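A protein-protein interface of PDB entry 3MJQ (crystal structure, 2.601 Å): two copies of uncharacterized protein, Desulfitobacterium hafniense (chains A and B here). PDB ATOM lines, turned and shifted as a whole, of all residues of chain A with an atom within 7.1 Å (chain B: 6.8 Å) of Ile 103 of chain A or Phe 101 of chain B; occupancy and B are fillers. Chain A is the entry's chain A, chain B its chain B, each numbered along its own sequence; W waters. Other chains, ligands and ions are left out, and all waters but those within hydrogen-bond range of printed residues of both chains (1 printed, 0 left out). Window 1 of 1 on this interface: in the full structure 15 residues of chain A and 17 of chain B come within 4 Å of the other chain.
Water W1 lies within hydrogen-bond range of the guanidinium group of Arg 88 of chain B (2.6 Å) and the guanidinium group of Arg 88 of chain A (3.3 Å).
O of Gly 92 of chain B sits at hydrogen-bond distance from N of Cys 99 of chain B. The backbone carbonyl oxygen of Trp 90 of chain B is in hydrogen-bond range of the backbone NH of Phe 101 of chain B, at 2.5 Å. The backbone NH (N) of Arg 88 of chain A sits at hydrogen-bond distance from the backbone carbonyl oxygen (O) of Ile 103 of chain A. The backbone NH (N) of Ile 14 of chain B sits at hydrogen-bond distance from the backbone carbonyl oxygen (O) of Tyr 23 of chain B, 3.1 Å away. O of Trp 90 of chain A sits at hydrogen-bond distance from N of Phe 101 of chain A (2.7 Å). The backbone carbonyl oxygen of Ile 103 of chain B sits at hydrogen-bond distance from the backbone NH of Arg 88 of chain B, at 2.8 Å.
Of the printed residues of chain B, Ile 103 of chain A touches Trp 90, Phe 101 and Ile 103. Of the printed residues of chain A, Phe 101 of chain B touches Phe 4 (3.4 Å), Ile 8 (3.8 Å) and Ile 103 (3.98 Å). Printed residues of chain B within 4 Å of Asp 10 of chain A: Trp 90 (3.4 Å). Of the printed residues of chain B, Phe 101 of chain A touches Ile 8. Of the printed residues of chain B, Trp 90 of chain A touches Ile 8 (3.9 Å), Trp 90 (3.5 Å) and Ile 103 (3.5 Å). Printed residues of chain B within 4 Å of Phe 4 of chain A: Ile 14 (3.7 Å), Cys 99 (3.4 Å) and Phe 101 (3.4 Å). Of the printed residues of chain A, Trp 90 of chain B touches Asp 10, Trp 90 and Ile 103. Leu 13 of chain A touches none of the printed residues of chain B. The nearest printed residue of chain A that does not touch Phe 101 of chain B is Leu 5 of chain A (4.5 Å).
Among the printed residues, pairs that only touch across the chains: Phe 4 of chain A with Ile 14 of chain B (3.7 Å), Phe 4 of chain A with Cys 99 of chain B (3.4 Å), Phe 4 of chain A with Phe 101 of chain B (3.4 Å), Ile 8 of chain A with Gln 91 of chain B (3.7 Å), Ile 8 of chain A with Phe 101 of chain B (3.8 Å), Trp 90 of chain A with Ile 8 of chain B (3.9 Å), Trp 90 of chain A with Trp 90 of chain B (3.5 Å), Trp 90 of chain A with Ile 103 of chain B (3.5 Å), Phe 101 of chain A with Ile 8 of chain B (3.4 Å), Ile 103 of chain A with Trp 90 of chain B (3.2 Å), Ile 103 of chain A with Phe 101 of chain B (3.98 Å) and Ile 103 of chain A with Ile 103 of chain B (3.7 Å).
Trp 90 of chain A touches Ile 8 of chain B, but with the chains exchanged Ile 8 of chain A does not touch Trp 90 of chain B (4.1 Å). Trp 90 of chain A touches its own counterpart, Trp 90 of chain B. Trp 90 of chain A touches Ile 103 of chain B, and with the chains exchanged Ile 103 of chain A touches Trp 90 of chain B. Ile 103 of chain A touches Phe 101 of chain B, but with the chains exchanged Phe 101 of chain A does not touch Ile 103 of chain B (4.01 Å). Positions printed for both chains: 5, 8, 12, 13, 88, 89, 90, 101, 102 and 103.
Printed residues of chain B that touch a printed residue of chain A: Ile 8, Ile 14, Arg 88, Trp 90, Gln 91, Cys 99, Phe 101 and Ile 103. Of the 17 printed residues of chain A, 7 touch a printed residue of chain B.
The guanidinium group of Arg 88 of chain A sits close to the guanidinium group of Arg 88 of chain B, 3.0 Å away. OD2 of Asp 10 of chain A sits at hydrogen-bond distance from NE1 of Trp 90 of chain B, 3.4 Å away.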
ATOM      1  N   PHE A   4       8.029  -9.211  -4.430  1.00  0.00           N
ATOM      2  CA  PHE A   4       8.850  -9.036  -3.247  1.00  0.00           C
ATOM      3  C   PHE A   4       9.681  -7.755  -3.347  1.00  0.00           C
ATOM      4  O   PHE A   4       9.431  -6.813  -2.610  1.00  0.00           O
ATOM      5  CB  PHE A   4       9.787 -10.233  -3.082  1.00  0.00           C
ATOM      6  CG  PHE A   4      10.707 -10.114  -1.903  1.00  0.00           C
ATOM      7  CD1 PHE A   4      10.207 -10.135  -0.607  1.00  0.00           C
ATOM      8  CD2 PHE A   4      12.073  -9.954  -2.088  1.00  0.00           C
ATOM      9  CE1 PHE A   4      11.057  -9.993   0.498  1.00  0.00           C
ATOM     10  CE2 PHE A   4      12.939  -9.809  -0.996  1.00  0.00           C
ATOM     11  CZ  PHE A   4      12.431  -9.828   0.302  1.00  0.00           C
ATOM     12  N   LEU A   5      10.680  -7.747  -4.239  1.00  0.00           N
ATOM     13  CA  LEU A   5      11.576  -6.604  -4.499  1.00  0.00           C
ATOM     14  C   LEU A   5      10.877  -5.248  -4.390  1.00  0.00           C
ATOM     15  O   LEU A   5      11.442  -4.289  -3.884  1.00  0.00           O
ATOM     16  CB  LEU A   5      12.181  -6.750  -5.893  1.00  0.00           C
ATOM     17  CG  LEU A   5      12.876  -8.103  -6.055  1.00  0.00           C
ATOM     18  CD1 LEU A   5      13.494  -8.176  -7.435  1.00  0.00           C
ATOM     19  CD2 LEU A   5      13.912  -8.300  -4.942  1.00  0.00           C
ATOM     20  N   ILE A   8      11.243  -3.252  -1.178  1.00  0.00           N
ATOM     21  CA  ILE A   8      12.515  -2.786  -0.639  1.00  0.00           C
ATOM     22  C   ILE A   8      12.647  -1.300  -0.963  1.00  0.00           C
ATOM     23  O   ILE A   8      12.371  -0.879  -2.085  1.00  0.00           O
ATOM     24  CB  ILE A   8      13.649  -3.603  -1.237  1.00  0.00           C
ATOM     25  CG1 ILE A   8      13.459  -5.068  -0.819  1.00  0.00           C
ATOM     26  CG2 ILE A   8      14.983  -3.037  -0.807  1.00  0.00           C
ATOM     27  CD1 ILE A   8      14.508  -6.020  -1.302  1.00  0.00           C
ATOM     28  N   ASP A  10      15.253   0.492  -1.279  1.00  0.00           N
ATOM     29  CA  ASP A  10      16.336   0.769  -2.206  1.00  0.00           C
ATOM     30  C   ASP A  10      15.923   0.490  -3.645  1.00  0.00           C
ATOM     31  O   ASP A  10      15.139  -0.418  -3.919  1.00  0.00           O
ATOM     32  CB  ASP A  10      17.558  -0.073  -1.858  1.00  0.00           C
ATOM     33  CG  ASP A  10      18.342   0.489  -0.690  1.00  0.00           C
ATOM     34  OD1 ASP A  10      17.762   1.242   0.122  1.00  0.00           O
ATOM     35  OD2 ASP A  10      19.545   0.163  -0.577  1.00  0.00           O
ATOM     36  N   MET A  11      16.479   1.275  -4.562  1.00  0.00           N
ATOM     37  CA  MET A  11      16.187   1.150  -5.981  1.00  0.00           C
ATOM     38  C   MET A  11      16.805  -0.120  -6.577  1.00  0.00           C
ATOM     39  O   MET A  11      17.999  -0.400  -6.420  1.00  0.00           O
ATOM     40  CB  MET A  11      16.689   2.388  -6.733  1.00  0.00           C
ATOM     41  CG  MET A  11      16.054   3.708  -6.327  1.00  0.00           C
ATOM     42  SD  MET A  11      16.956   5.232  -7.138  1.00  0.00           S
ATOM     43  CE  MET A  11      18.456   5.386  -5.882  1.00  0.00           C
ATOM     44  N   ILE A  12      15.963  -0.895  -7.251  1.00  0.00           N
ATOM     45  CA  ILE A  12      16.404  -2.124  -7.857  1.00  0.00           C
ATOM     46  C   ILE A  12      16.026  -2.080  -9.302  1.00  0.00           C
ATOM     47  O   ILE A  12      14.885  -1.791  -9.644  1.00  0.00           O
ATOM     48  CB  ILE A  12      15.733  -3.359  -7.239  1.00  0.00           C
ATOM     49  CG1 ILE A  12      16.270  -3.608  -5.830  1.00  0.00           C
ATOM     50  CG2 ILE A  12      15.986  -4.579  -8.126  1.00  0.00           C
ATOM     51  CD1 ILE A  12      15.549  -4.716  -5.103  1.00  0.00           C
ATOM     52  N   LEU A  13      17.005  -2.374 -10.142  1.00  0.00           N
ATOM     53  CA  LEU A  13      16.824  -2.393 -11.578  1.00  0.00           C
ATOM     54  C   LEU A  13      17.484  -3.653 -12.089  1.00  0.00           C
ATOM     55  O   LEU A  13      18.407  -4.179 -11.465  1.00  0.00           O
ATOM     56  CB  LEU A  13      17.526  -1.197 -12.233  1.00  0.00           C
ATOM     57  CG  LEU A  13      17.206   0.237 -11.805  1.00  0.00           C
ATOM     58  CD1 LEU A  13      18.187   1.188 -12.482  1.00  0.00           C
ATOM     59  CD2 LEU A  13      15.769   0.612 -12.186  1.00  0.00           C
ATOM     60  N   LYS A  86      25.166   4.682  -4.536  1.00  0.00           N
ATOM     61  CA  LYS A  86      26.110   3.593  -4.527  1.00  0.00           C
ATOM     62  C   LYS A  86      25.297   2.412  -5.029  1.00  0.00           C
ATOM     63  O   LYS A  86      24.212   2.110  -4.520  1.00  0.00           O
ATOM     64  CB  LYS A  86      26.665   3.313  -3.126  1.00  0.00           C
ATOM     65  CG  LYS A  86      27.743   2.226  -3.150  1.00  0.00           C
ATOM     66  CD  LYS A  86      28.486   2.091  -1.832  1.00  0.00           C
ATOM     67  CE  LYS A  86      29.701   1.167  -1.983  1.00  0.00           C
ATOM     68  NZ  LYS A  86      30.453   0.952  -0.703  1.00  0.00           N
ATOM     69  N   ALA A  87      25.811   1.762  -6.061  1.00  0.00           N
ATOM     70  CA  ALA A  87      25.101   0.638  -6.622  1.00  0.00           C
ATOM     71  C   ALA A  87      25.887  -0.646  -6.477  1.00  0.00           C
ATOM     72  O   ALA A  87      27.080  -0.680  -6.742  1.00  0.00           O
ATOM     73  CB  ALA A  87      24.807   0.905  -8.079  1.00  0.00           C
ATOM     74  N   ARG A  88      25.215  -1.695  -6.025  1.00  0.00           N
ATOM     75  CA  ARG A  88      25.828  -3.004  -5.905  1.00  0.00           C
ATOM     76  C   ARG A  88      25.191  -3.818  -7.027  1.00  0.00           C
ATOM     77  O   ARG A  88      23.956  -3.778  -7.225  1.00  0.00           O
ATOM     78  CB  ARG A  88      25.523  -3.612  -4.536  1.00  0.00           C
ATOM     79  CG  ARG A  88      26.242  -2.868  -3.422  1.00  0.00           C
ATOM     80  CD  ARG A  88      25.659  -3.107  -2.037  1.00  0.00           C
ATOM     81  NE  ARG A  88      26.040  -2.039  -1.108  1.00  0.00           N
ATOM     82  CZ  ARG A  88      27.287  -1.797  -0.714  1.00  0.00           C
ATOM     83  NH1 ARG A  88      28.285  -2.553  -1.162  1.00  0.00           N
ATOM     84  NH2 ARG A  88      27.534  -0.785   0.114  1.00  0.00           N
ATOM     85  N   ILE A  89      26.032  -4.522  -7.784  1.00  0.00           N
ATOM     86  CA  ILE A  89      25.536  -5.319  -8.895  1.00  0.00           C
ATOM     87  C   ILE A  89      25.904  -6.800  -8.862  1.00  0.00           C
ATOM     88  O   ILE A  89      26.959  -7.191  -8.365  1.00  0.00           O
ATOM     89  CB  ILE A  89      25.976  -4.720 -10.247  1.00  0.00           C
ATOM     90  CG1 ILE A  89      27.440  -5.040 -10.515  1.00  0.00           C
ATOM     91  CG2 ILE A  89      25.775  -3.200 -10.246  1.00  0.00           C
ATOM     92  CD1 ILE A  89      27.875  -4.641 -11.909  1.00  0.00           C
ATOM     93  N   TRP A  90      24.988  -7.611  -9.384  1.00  0.00           N
ATOM     94  CA  TRP A  90      25.134  -9.052  -9.461  1.00  0.00           C
ATOM     95  C   TRP A  90      24.790  -9.458 -10.873  1.00  0.00           C
ATOM     96  O   TRP A  90      23.846  -8.938 -11.461  1.00  0.00           O
ATOM     97  CB  TRP A  90      24.183  -9.743  -8.485  1.00  0.00           C
ATOM     98  CG  TRP A  90      24.619  -9.629  -7.064  1.00  0.00           C
ATOM     99  CD1 TRP A  90      25.465 -10.466  -6.395  1.00  0.00           C
ATOM    100  CD2 TRP A  90      24.294  -8.573  -6.154  1.00  0.00           C
ATOM    101  NE1 TRP A  90      25.689  -9.993  -5.129  1.00  0.00           N
ATOM    102  CE2 TRP A  90      24.983  -8.833  -4.954  1.00  0.00           C
ATOM    103  CE3 TRP A  90      23.485  -7.431  -6.241  1.00  0.00           C
ATOM    104  CZ2 TRP A  90      24.892  -7.990  -3.842  1.00  0.00           C
ATOM    105  CZ3 TRP A  90      23.398  -6.594  -5.136  1.00  0.00           C
ATOM    106  CH2 TRP A  90      24.101  -6.881  -3.952  1.00  0.00           C
ATOM    107  N   PHE A 101      21.921  -7.259 -12.237  1.00  0.00           N
ATOM    108  CA  PHE A 101      20.940  -7.083 -11.170  1.00  0.00           C
ATOM    109  C   PHE A 101      21.530  -6.029 -10.246  1.00  0.00           C
ATOM    110  O   PHE A 101      22.579  -6.234  -9.646  1.00  0.00           O
ATOM    111  CB  PHE A 101      20.723  -8.381 -10.403  1.00  0.00           C
ATOM    112  CG  PHE A 101      19.837  -8.227  -9.205  1.00  0.00           C
ATOM    113  CD1 PHE A 101      18.568  -7.673  -9.336  1.00  0.00           C
ATOM    114  CD2 PHE A 101      20.261  -8.640  -7.949  1.00  0.00           C
ATOM    115  CE1 PHE A 101      17.734  -7.532  -8.232  1.00  0.00           C
ATOM    116  CE2 PHE A 101      19.432  -8.502  -6.843  1.00  0.00           C
ATOM    117  CZ  PHE A 101      18.165  -7.946  -6.989  1.00  0.00           C
ATOM    118  N   ALA A 102      20.850  -4.899 -10.124  1.00  0.00           N
ATOM    119  CA  ALA A 102      21.380  -3.822  -9.313  1.00  0.00           C
ATOM    120  C   ALA A 102      20.480  -3.311  -8.206  1.00  0.00           C
ATOM    121  O   ALA A 102      19.282  -3.064  -8.403  1.00  0.00           O
ATOM    122  CB  ALA A 102      21.768  -2.661 -10.213  1.00  0.00           C
ATOM    123  N   ILE A 103      21.090  -3.146  -7.038  1.00  0.00           N
ATOM    124  CA  ILE A 103      20.404  -2.612  -5.879  1.00  0.00           C
ATOM    125  C   ILE A 103      21.193  -1.333  -5.591  1.00  0.00           C
ATOM    126  O   ILE A 103      22.405  -1.366  -5.347  1.00  0.00           O
ATOM    127  CB  ILE A 103      20.445  -3.603  -4.693  1.00  0.00           C
ATOM    128  CG1 ILE A 103      19.996  -4.995  -5.190  1.00  0.00           C
ATOM    129  CG2 ILE A 103      19.543  -3.095  -3.551  1.00  0.00           C
ATOM    130  CD1 ILE A 103      19.908  -6.079  -4.121  1.00  0.00           C
ATOM    131  N   ILE A 104      20.489  -0.207  -5.657  1.00  0.00           N
ATOM    132  CA  ILE A 104      21.098   1.096  -5.474  1.00  0.00           C
ATOM    133  C   ILE A 104      20.701   1.860  -4.220  1.00  0.00           C
ATOM    134  O   ILE A 104      19.513   2.076  -3.967  1.00  0.00           O
ATOM    135  CB  ILE A 104      20.784   1.946  -6.685  1.00  0.00           C
ATOM    136  CG1 ILE A 104      21.195   1.157  -7.927  1.00  0.00           C
ATOM    137  CG2 ILE A 104      21.523   3.283  -6.613  1.00  0.00           C
ATOM    138  CD1 ILE A 104      20.571   1.659  -9.188  1.00  0.00           C
ATOM    139  N   LYS A 105      21.714   2.279  -3.451  1.00  0.00           N
ATOM    140  CA  LYS A 105      21.520   3.047  -2.216  1.00  0.00           C
ATOM    141  C   LYS A 105      21.683   4.556  -2.433  1.00  0.00           C
ATOM    142  O   LYS A 105      22.730   5.030  -2.893  1.00  0.00           O
ATOM    143  CB  LYS A 105      22.501   2.593  -1.128  1.00  0.00           C
ATOM    144  CG  LYS A 105      22.337   3.342   0.193  1.00  0.00           C
ATOM    145  CD  LYS A 105      23.286   2.844   1.273  1.00  0.00           C
ATOM    146  CE  LYS A 105      23.151   3.684   2.527  1.00  0.00           C
ATOM    147  NZ  LYS A 105      24.267   3.423   3.458  1.00  0.00           N
ATOM    148  N   LEU B   5      16.320 -14.786  -9.169  1.00  0.00           N
ATOM    149  CA  LEU B   5      17.332 -14.875  -8.110  1.00  0.00           C
ATOM    150  C   LEU B   5      18.028 -16.224  -8.193  1.00  0.00           C
ATOM    151  O   LEU B   5      19.187 -16.373  -7.801  1.00  0.00           O
ATOM    152  CB  LEU B   5      16.657 -14.739  -6.752  1.00  0.00           C
ATOM    153  CG  LEU B   5      15.760 -13.505  -6.608  1.00  0.00           C
ATOM    154  CD1 LEU B   5      15.183 -13.466  -5.192  1.00  0.00           C
ATOM    155  CD2 LEU B   5      16.553 -12.234  -6.960  1.00  0.00           C
ATOM    156  N   ILE B   8      21.473 -16.097  -9.663  1.00  0.00           N
ATOM    157  CA  ILE B   8      22.604 -15.367  -9.102  1.00  0.00           C
ATOM    158  C   ILE B   8      23.501 -16.335  -8.341  1.00  0.00           C
ATOM    159  O   ILE B   8      23.027 -17.135  -7.540  1.00  0.00           O
ATOM    160  CB  ILE B   8      22.133 -14.201  -8.187  1.00  0.00           C
ATOM    161  CG1 ILE B   8      21.474 -13.121  -9.055  1.00  0.00           C
ATOM    162  CG2 ILE B   8      23.315 -13.608  -7.415  1.00  0.00           C
ATOM    163  CD1 ILE B   8      20.870 -11.969  -8.295  1.00  0.00           C
ATOM    164  N   ILE B  12      21.375 -16.321  -1.548  1.00  0.00           N
ATOM    165  CA  ILE B  12      20.286 -15.408  -1.244  1.00  0.00           C
ATOM    166  C   ILE B  12      19.261 -16.050  -0.292  1.00  0.00           C
ATOM    167  O   ILE B  12      18.831 -17.194  -0.493  1.00  0.00           O
ATOM    168  CB  ILE B  12      19.562 -14.956  -2.533  1.00  0.00           C
ATOM    169  CG1 ILE B  12      20.550 -14.292  -3.493  1.00  0.00           C
ATOM    170  CG2 ILE B  12      18.419 -14.007  -2.174  1.00  0.00           C
ATOM    171  CD1 ILE B  12      19.894 -13.696  -4.723  1.00  0.00           C
ATOM    172  N   LEU B  13      18.879 -15.295   0.739  1.00  0.00           N
ATOM    173  CA  LEU B  13      17.921 -15.748   1.752  1.00  0.00           C
ATOM    174  C   LEU B  13      16.887 -14.678   2.108  1.00  0.00           C
ATOM    175  O   LEU B  13      17.215 -13.492   2.169  1.00  0.00           O
ATOM    176  CB  LEU B  13      18.641 -16.093   3.066  1.00  0.00           C
ATOM    177  CG  LEU B  13      19.660 -17.207   3.256  1.00  0.00           C
ATOM    178  CD1 LEU B  13      20.228 -17.118   4.674  1.00  0.00           C
ATOM    179  CD2 LEU B  13      18.997 -18.558   3.034  1.00  0.00           C
ATOM    180  N   ILE B  14      15.641 -15.100   2.323  1.00  0.00           N
ATOM    181  CA  ILE B  14      14.612 -14.187   2.810  1.00  0.00           C
ATOM    182  C   ILE B  14      14.381 -14.760   4.219  1.00  0.00           C
ATOM    183  O   ILE B  14      14.083 -15.943   4.381  1.00  0.00           O
ATOM    184  CB  ILE B  14      13.303 -14.218   1.991  1.00  0.00           C
ATOM    185  CG1 ILE B  14      13.437 -13.371   0.723  1.00  0.00           C
ATOM    186  CG2 ILE B  14      12.175 -13.601   2.816  1.00  0.00           C
ATOM    187  CD1 ILE B  14      14.370 -13.920  -0.283  1.00  0.00           C
ATOM    188  N   ILE B  15      14.547 -13.924   5.234  1.00  0.00           N
ATOM    189  CA  ILE B  15      14.424 -14.361   6.624  1.00  0.00           C
ATOM    190  C   ILE B  15      13.327 -13.577   7.353  1.00  0.00           C
ATOM    191  O   ILE B  15      13.191 -12.376   7.150  1.00  0.00           O
ATOM    192  CB  ILE B  15      15.797 -14.134   7.333  1.00  0.00           C
ATOM    193  CG1 ILE B  15      16.866 -15.001   6.672  1.00  0.00           C
ATOM    194  CG2 ILE B  15      15.702 -14.402   8.816  1.00  0.00           C
ATOM    195  CD1 ILE B  15      18.229 -14.337   6.590  1.00  0.00           C
ATOM    196  N   TYR B  23      12.686 -18.304   2.308  1.00  0.00           N
ATOM    197  CA  TYR B  23      13.160 -18.538   0.962  1.00  0.00           C
ATOM    198  C   TYR B  23      14.665 -18.652   0.923  1.00  0.00           C
ATOM    199  O   TYR B  23      15.370 -18.121   1.775  1.00  0.00           O
ATOM    200  CB  TYR B  23      12.728 -17.397   0.037  1.00  0.00           C
ATOM    201  CG  TYR B  23      13.353 -17.496  -1.327  1.00  0.00           C
ATOM    202  CD1 TYR B  23      12.783 -18.283  -2.318  1.00  0.00           C
ATOM    203  CD2 TYR B  23      14.567 -16.866  -1.601  1.00  0.00           C
ATOM    204  CE1 TYR B  23      13.407 -18.449  -3.552  1.00  0.00           C
ATOM    205  CE2 TYR B  23      15.205 -17.025  -2.829  1.00  0.00           C
ATOM    206  CZ  TYR B  23      14.620 -17.818  -3.800  1.00  0.00           C
ATOM    207  OH  TYR B  23      15.256 -17.992  -5.007  1.00  0.00           O
ATOM    208  N   ARG B  88      24.961  -9.089   2.911  1.00  0.00           N
ATOM    209  CA  ARG B  88      24.457  -7.759   2.608  1.00  0.00           C
ATOM    210  C   ARG B  88      22.956  -7.892   2.816  1.00  0.00           C
ATOM    211  O   ARG B  88      22.308  -8.740   2.193  1.00  0.00           O
ATOM    212  CB  ARG B  88      24.824  -7.389   1.169  1.00  0.00           C
ATOM    213  CG  ARG B  88      26.343  -7.480   0.952  1.00  0.00           C
ATOM    214  CD  ARG B  88      26.866  -6.772  -0.295  1.00  0.00           C
ATOM    215  NE  ARG B  88      28.323  -6.610  -0.240  1.00  0.00           N
ATOM    216  CZ  ARG B  88      28.947  -5.597   0.357  1.00  0.00           C
ATOM    217  NH1 ARG B  88      28.248  -4.633   0.949  1.00  0.00           N
ATOM    218  NH2 ARG B  88      30.274  -5.552   0.366  1.00  0.00           N
ATOM    219  N   ILE B  89      22.400  -7.093   3.718  1.00  0.00           N
ATOM    220  CA  ILE B  89      20.978  -7.230   3.981  1.00  0.00           C
ATOM    221  C   ILE B  89      20.102  -6.008   3.697  1.00  0.00           C
ATOM    222  O   ILE B  89      20.523  -4.862   3.848  1.00  0.00           O
ATOM    223  CB  ILE B  89      20.728  -7.738   5.452  1.00  0.00           C
ATOM    224  CG1 ILE B  89      20.943  -6.620   6.461  1.00  0.00           C
ATOM    225  CG2 ILE B  89      21.698  -8.863   5.806  1.00  0.00           C
ATOM    226  CD1 ILE B  89      19.761  -5.650   6.590  1.00  0.00           C
ATOM    227  N   TRP B  90      18.872  -6.283   3.283  1.00  0.00           N
ATOM    228  CA  TRP B  90      17.885  -5.262   2.971  1.00  0.00           C
ATOM    229  C   TRP B  90      16.568  -5.635   3.650  1.00  0.00           C
ATOM    230  O   TRP B  90      16.234  -6.810   3.773  1.00  0.00           O
ATOM    231  CB  TRP B  90      17.672  -5.205   1.472  1.00  0.00           C
ATOM    232  CG  TRP B  90      18.800  -4.630   0.726  1.00  0.00           C
ATOM    233  CD1 TRP B  90      18.951  -3.332   0.367  1.00  0.00           C
ATOM    234  CD2 TRP B  90      19.924  -5.335   0.184  1.00  0.00           C
ATOM    235  NE1 TRP B  90      20.090  -3.177  -0.380  1.00  0.00           N
ATOM    236  CE2 TRP B  90      20.711  -4.390  -0.506  1.00  0.00           C
ATOM    237  CE3 TRP B  90      20.340  -6.672   0.209  1.00  0.00           C
ATOM    238  CZ2 TRP B  90      21.893  -4.731  -1.165  1.00  0.00           C
ATOM    239  CZ3 TRP B  90      21.523  -7.012  -0.453  1.00  0.00           C
ATOM    240  CH2 TRP B  90      22.282  -6.039  -1.129  1.00  0.00           C
ATOM    241  N   GLN B  91      15.827  -4.637   4.100  1.00  0.00           N
ATOM    242  CA  GLN B  91      14.557  -4.893   4.745  1.00  0.00           C
ATOM    243  C   GLN B  91      13.482  -4.849   3.685  1.00  0.00           C
ATOM    244  O   GLN B  91      13.548  -4.050   2.750  1.00  0.00           O
ATOM    245  CB  GLN B  91      14.288  -3.845   5.815  1.00  0.00           C
ATOM    246  CG  GLN B  91      15.260  -3.926   6.978  1.00  0.00           C
ATOM    247  CD  GLN B  91      15.344  -2.630   7.748  1.00  0.00           C
ATOM    248  OE1 GLN B  91      15.090  -2.588   8.955  1.00  0.00           O
ATOM    249  NE2 GLN B  91      15.705  -1.558   7.053  1.00  0.00           N
ATOM    250  N   GLY B  92      12.503  -5.734   3.828  1.00  0.00           N
ATOM    251  CA  GLY B  92      11.394  -5.805   2.896  1.00  0.00           C
ATOM    252  C   GLY B  92      10.222  -6.468   3.592  1.00  0.00           C
ATOM    253  O   GLY B  92      10.247  -6.660   4.810  1.00  0.00           O
ATOM    254  N   CYS B  99      10.512  -8.718   6.808  1.00  0.00           N
ATOM    255  CA  CYS B  99      11.512  -9.738   6.583  1.00  0.00           C
ATOM    256  C   CYS B  99      12.832  -9.087   6.148  1.00  0.00           C
ATOM    257  O   CYS B  99      12.871  -7.909   5.776  1.00  0.00           O
ATOM    258  CB  CYS B  99      11.036 -10.713   5.512  1.00  0.00           C
ATOM    259  SG  CYS B  99      11.019  -9.948   3.904  1.00  0.00           S
ATOM    260  N   LEU B 100      13.902  -9.870   6.215  1.00  0.00           N
ATOM    261  CA  LEU B 100      15.228  -9.447   5.809  1.00  0.00           C
ATOM    262  C   LEU B 100      15.578 -10.128   4.477  1.00  0.00           C
ATOM    263  O   LEU B 100      15.366 -11.333   4.302  1.00  0.00           O
ATOM    264  CB  LEU B 100      16.241  -9.853   6.881  1.00  0.00           C
ATOM    265  CG  LEU B 100      16.917  -8.759   7.711  1.00  0.00           C
ATOM    266  CD1 LEU B 100      15.969  -7.599   7.943  1.00  0.00           C
ATOM    267  CD2 LEU B 100      17.402  -9.365   9.033  1.00  0.00           C
ATOM    268  N   PHE B 101      16.070  -9.339   3.528  1.00  0.00           N
ATOM    269  CA  PHE B 101      16.504  -9.863   2.233  1.00  0.00           C
ATOM    270  C   PHE B 101      18.034  -9.854   2.283  1.00  0.00           C
ATOM    271  O   PHE B 101      18.660  -8.801   2.440  1.00  0.00           O
ATOM    272  CB  PHE B 101      16.032  -8.976   1.095  1.00  0.00           C
ATOM    273  CG  PHE B 101      16.552  -9.396  -0.243  1.00  0.00           C
ATOM    274  CD1 PHE B 101      16.238 -10.648  -0.773  1.00  0.00           C
ATOM    275  CD2 PHE B 101      17.332  -8.529  -1.001  1.00  0.00           C
ATOM    276  CE1 PHE B 101      16.693 -11.038  -2.056  1.00  0.00           C
ATOM    277  CE2 PHE B 101      17.793  -8.907  -2.279  1.00  0.00           C
ATOM    278  CZ  PHE B 101      17.465 -10.168  -2.806  1.00  0.00           C
ATOM    279  N   ALA B 102      18.641 -11.025   2.148  1.00  0.00           N
ATOM    280  CA  ALA B 102      20.084 -11.106   2.236  1.00  0.00           C
ATOM    281  C   ALA B 102      20.772 -11.758   1.070  1.00  0.00           C
ATOM    282  O   ALA B 102      20.380 -12.825   0.612  1.00  0.00           O
ATOM    283  CB  ALA B 102      20.465 -11.829   3.509  1.00  0.00           C
ATOM    284  N   ILE B 103      21.805 -11.091   0.587  1.00  0.00           N
ATOM    285  CA  ILE B 103      22.611 -11.623  -0.494  1.00  0.00           C
ATOM    286  C   ILE B 103      23.954 -11.787   0.192  1.00  0.00           C
ATOM    287  O   ILE B 103      24.542 -10.808   0.680  1.00  0.00           O
ATOM    288  CB  ILE B 103      22.701 -10.663  -1.683  1.00  0.00           C
ATOM    289  CG1 ILE B 103      21.290 -10.264  -2.127  1.00  0.00           C
ATOM    290  CG2 ILE B 103      23.406 -11.357  -2.841  1.00  0.00           C
ATOM    291  CD1 ILE B 103      21.247  -9.400  -3.377  1.00  0.00           C
HETATM  292  O   HOH W   1      25.800  -4.002   1.539  1.00  0.00           O
